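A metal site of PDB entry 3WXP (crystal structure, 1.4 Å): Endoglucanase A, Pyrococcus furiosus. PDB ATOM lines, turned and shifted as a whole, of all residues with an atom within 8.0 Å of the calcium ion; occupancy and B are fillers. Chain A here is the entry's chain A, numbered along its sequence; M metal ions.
The side-chain carboxylate of Glu 76 sits at hydrogen-bond distance from the backbone NH of Lys 69 (2.7 Å).
The backbone NH of Glu 76 lies within hydrogen-bond range of the backbone carbonyl oxygen of Ile 67 (2.8 Å).
The side-chain amide oxygen (OD1) of Asn 74 lies within hydrogen-bond range of the side-chain hydroxyl (OG1) of Thr 141 (2.7 Å).
N of Asp 142 sits at hydrogen-bond distance from O of Pro 75, 3.0 Å away.
The side-chain carboxylate of Asp 68 sits close to the backbone NH of Gly 71, 3.4 Å away.
OD2 of Asp 68 lies within hydrogen-bond range of N of Gly 73.
Six residues have an atom within 4 Å of the calcium ion: Asp 68, Asp 70, Asp 72, Asn 74, Glu 76 and Asp 142.
The calcium ion is bound by the side-chain carboxylate (OD1) of Asp 70 (2.3 Å).
OE2 of Glu 76 is bound to the calcium ion (2.3 Å).
The backbone carbonyl oxygen (O) of Asn 74 is bound to the calcium ion (2.4 Å).
The calcium ion is bound by OD2 of Asp 142.
OD1 of Asp 72 binds the calcium ion, 2.4 Å away.
The calcium ion is bound by OD1 of Asp 68 (2.4 Å).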
ATOM      1  N   ILE A  67      -2.515 -14.004  27.358  1.00  0.00           N
ATOM      2  CA  ILE A  67      -1.842 -14.323  26.074  1.00  0.00           C
ATOM      3  C   ILE A  67      -2.442 -13.370  25.084  1.00  0.00           C
ATOM      4  O   ILE A  67      -3.650 -13.440  24.801  1.00  0.00           O
ATOM      5  CB  ILE A  67      -2.066 -15.787  25.656  1.00  0.00           C
ATOM      6  CG1 ILE A  67      -1.293 -16.667  26.692  1.00  0.00           C
ATOM      7  CG2 ILE A  67      -1.549 -16.014  24.214  1.00  0.00           C
ATOM      8  CD1 ILE A  67      -1.560 -18.160  26.508  1.00  0.00           C
ATOM      9  N   ASP A  68      -1.628 -12.463  24.522  1.00  0.00           N
ATOM     10  CA  ASP A  68      -2.133 -11.433  23.639  1.00  0.00           C
ATOM     11  C   ASP A  68      -1.158 -11.323  22.483  1.00  0.00           C
ATOM     12  O   ASP A  68      -0.311 -10.390  22.451  1.00  0.00           O
ATOM     13  CB  ASP A  68      -2.280 -10.134  24.456  1.00  0.00           C
ATOM     14  CG  ASP A  68      -2.883  -8.960  23.634  1.00  0.00           C
ATOM     15  OD1 ASP A  68      -3.480  -9.198  22.561  1.00  0.00           O
ATOM     16  OD2 ASP A  68      -2.792  -7.791  24.124  1.00  0.00           O
ATOM     17  N   LYS A  69      -1.253 -12.252  21.527  1.00  0.00           N
ATOM     18  CA  LYS A  69      -0.164 -12.400  20.553  1.00  0.00           C
ATOM     19  C   LYS A  69      -0.047 -11.161  19.624  1.00  0.00           C
ATOM     20  O   LYS A  69       1.013 -10.857  19.110  1.00  0.00           O
ATOM     21  CB  LYS A  69      -0.307 -13.691  19.765  1.00  0.00           C
ATOM     22  CG  LYS A  69      -1.483 -13.708  18.821  1.00  0.00           C
ATOM     23  CD  LYS A  69      -1.506 -14.953  17.920  1.00  0.00           C
ATOM     24  CE  LYS A  69      -2.934 -15.187  17.393  1.00  0.00           C
ATOM     25  NZ  LYS A  69      -3.689 -13.888  17.413  1.00  0.00           N
ATOM     26  N   ASP A  70      -1.165 -10.462  19.376  1.00  0.00           N
ATOM     27  CA  ASP A  70      -1.163  -9.308  18.477  1.00  0.00           C
ATOM     28  C   ASP A  70      -1.011  -8.025  19.253  1.00  0.00           C
ATOM     29  O   ASP A  70      -1.015  -6.941  18.643  1.00  0.00           O
ATOM     30  CB  ASP A  70      -2.374  -9.329  17.558  1.00  0.00           C
ATOM     31  CG  ASP A  70      -3.720  -9.198  18.305  1.00  0.00           C
ATOM     32  OD1 ASP A  70      -3.796  -9.403  19.534  1.00  0.00           O
ATOM     33  OD2 ASP A  70      -4.772  -8.917  17.634  1.00  0.00           O
ATOM     34  N   GLY A  71      -0.885  -8.125  20.599  1.00  0.00           N
ATOM     35  CA  GLY A  71      -0.611  -6.946  21.439  1.00  0.00           C
ATOM     36  C   GLY A  71      -1.726  -5.887  21.361  1.00  0.00           C
ATOM     37  O   GLY A  71      -1.444  -4.655  21.593  1.00  0.00           O
ATOM     38  N   ASP A  72      -2.976  -6.326  21.169  1.00  0.00           N
ATOM     39  CA  ASP A  72      -4.071  -5.342  20.932  1.00  0.00           C
ATOM     40  C   ASP A  72      -4.835  -5.078  22.223  1.00  0.00           C
ATOM     41  O   ASP A  72      -5.803  -4.284  22.178  1.00  0.00           O
ATOM     42  CB  ASP A  72      -4.978  -5.737  19.765  1.00  0.00           C
ATOM     43  CG  ASP A  72      -6.003  -6.869  20.132  1.00  0.00           C
ATOM     44  OD1 ASP A  72      -5.796  -7.563  21.156  1.00  0.00           O
ATOM     45  OD2 ASP A  72      -6.995  -7.055  19.345  1.00  0.00           O
ATOM     46  N   GLY A  73      -4.418  -5.621  23.368  1.00  0.00           N
ATOM     47  CA  GLY A  73      -5.081  -5.319  24.662  1.00  0.00           C
ATOM     48  C   GLY A  73      -6.288  -6.175  24.922  1.00  0.00           C
ATOM     49  O   GLY A  73      -6.940  -5.994  25.991  1.00  0.00           O
ATOM     50  N   ASN A  74      -6.622  -7.086  23.986  1.00  0.00           N
ATOM     51  CA  ASN A  74      -7.700  -8.055  24.233  1.00  0.00           C
ATOM     52  C   ASN A  74      -7.037  -9.450  24.151  1.00  0.00           C
ATOM     53  O   ASN A  74      -6.688  -9.872  23.071  1.00  0.00           O
ATOM     54  CB  ASN A  74      -8.736  -7.912  23.135  1.00  0.00           C
ATOM     55  CG  ASN A  74     -10.026  -8.661  23.486  1.00  0.00           C
ATOM     56  OD1 ASN A  74     -10.111  -9.273  24.596  1.00  0.00           O
ATOM     57  ND2 ASN A  74     -10.986  -8.695  22.553  1.00  0.00           N
ATOM     58  N   PRO A  75      -6.909 -10.143  25.290  1.00  0.00           N
ATOM     59  CA  PRO A  75      -6.136 -11.413  25.228  1.00  0.00           C
ATOM     60  C   PRO A  75      -6.927 -12.463  24.388  1.00  0.00           C
ATOM     61  O   PRO A  75      -8.184 -12.482  24.458  1.00  0.00           O
ATOM     62  CB  PRO A  75      -6.094 -11.823  26.728  1.00  0.00           C
ATOM     63  CG  PRO A  75      -6.180 -10.511  27.479  1.00  0.00           C
ATOM     64  CD  PRO A  75      -7.235  -9.782  26.680  1.00  0.00           C
ATOM     65  N   GLU A  76      -6.257 -13.379  23.700  1.00  0.00           N
ATOM     66  CA  GLU A  76      -6.896 -14.535  23.053  1.00  0.00           C
ATOM     67  C   GLU A  76      -7.193 -15.598  24.122  1.00  0.00           C
ATOM     68  O   GLU A  76      -8.182 -16.346  23.948  1.00  0.00           O
ATOM     69  CB  GLU A  76      -6.048 -15.165  21.936  1.00  0.00           C
ATOM     70  CG  GLU A  76      -5.698 -14.125  20.861  1.00  0.00           C
ATOM     71  CD  GLU A  76      -4.471 -13.312  21.177  1.00  0.00           C
ATOM     72  OE1 GLU A  76      -3.433 -13.881  21.545  1.00  0.00           O
ATOM     73  OE2 GLU A  76      -4.498 -12.041  21.077  1.00  0.00           O
ATOM     74  N   PHE A  77      -6.330 -15.729  25.143  1.00  0.00           N
ATOM     75  CA  PHE A  77      -6.524 -16.690  26.226  1.00  0.00           C
ATOM     76  C   PHE A  77      -5.915 -16.108  27.478  1.00  0.00           C
ATOM     77  O   PHE A  77      -5.175 -15.075  27.386  1.00  0.00           O
ATOM     78  CB  PHE A  77      -5.782 -18.011  25.957  1.00  0.00           C
ATOM     79  CG  PHE A  77      -6.353 -18.783  24.790  1.00  0.00           C
ATOM     80  CD1 PHE A  77      -7.536 -19.554  24.934  1.00  0.00           C
ATOM     81  CD2 PHE A  77      -5.737 -18.719  23.523  1.00  0.00           C
ATOM     82  CE1 PHE A  77      -8.099 -20.196  23.824  1.00  0.00           C
ATOM     83  CE2 PHE A  77      -6.268 -19.360  22.465  1.00  0.00           C
ATOM     84  CZ  PHE A  77      -7.457 -20.133  22.590  1.00  0.00           C
ATOM     85  N   THR A 141     -11.085 -12.195  25.458  1.00  0.00           N
ATOM     86  CA  THR A 141     -12.234 -12.204  24.590  1.00  0.00           C
ATOM     87  C   THR A 141     -11.892 -12.057  23.090  1.00  0.00           C
ATOM     88  O   THR A 141     -12.778 -11.830  22.270  1.00  0.00           O
ATOM     89  CB  THR A 141     -13.300 -11.165  25.009  1.00  0.00           C
ATOM     90  OG1 THR A 141     -12.763  -9.844  24.882  1.00  0.00           O
ATOM     91  CG2 THR A 141     -13.806 -11.435  26.443  1.00  0.00           C
ATOM     92  N   ASP A 142     -10.606 -12.215  22.731  1.00  0.00           N
ATOM     93  CA  ASP A 142     -10.182 -12.071  21.320  1.00  0.00           C
ATOM     94  C   ASP A 142     -10.313 -13.498  20.715  1.00  0.00           C
ATOM     95  O   ASP A 142      -9.309 -14.245  20.668  1.00  0.00           O
ATOM     96  CB  ASP A 142      -8.764 -11.535  21.312  1.00  0.00           C
ATOM     97  CG  ASP A 142      -8.289 -11.169  19.920  1.00  0.00           C
ATOM     98  OD1 ASP A 142      -8.997 -11.407  18.910  1.00  0.00           O
ATOM     99  OD2 ASP A 142      -7.137 -10.592  19.885  1.00  0.00           O
ATOM    100  N   GLY A 143     -11.525 -13.867  20.287  1.00  0.00           N
ATOM    101  CA  GLY A 143     -11.792 -15.206  19.710  1.00  0.00           C
ATOM    102  C   GLY A 143     -13.080 -15.203  18.932  1.00  0.00           C
ATOM    103  O   GLY A 143     -13.826 -14.179  18.971  1.00  0.00           O
HETATM  104 CA    CA M   1      -5.282  -9.880  21.175  1.00  0.00          CA
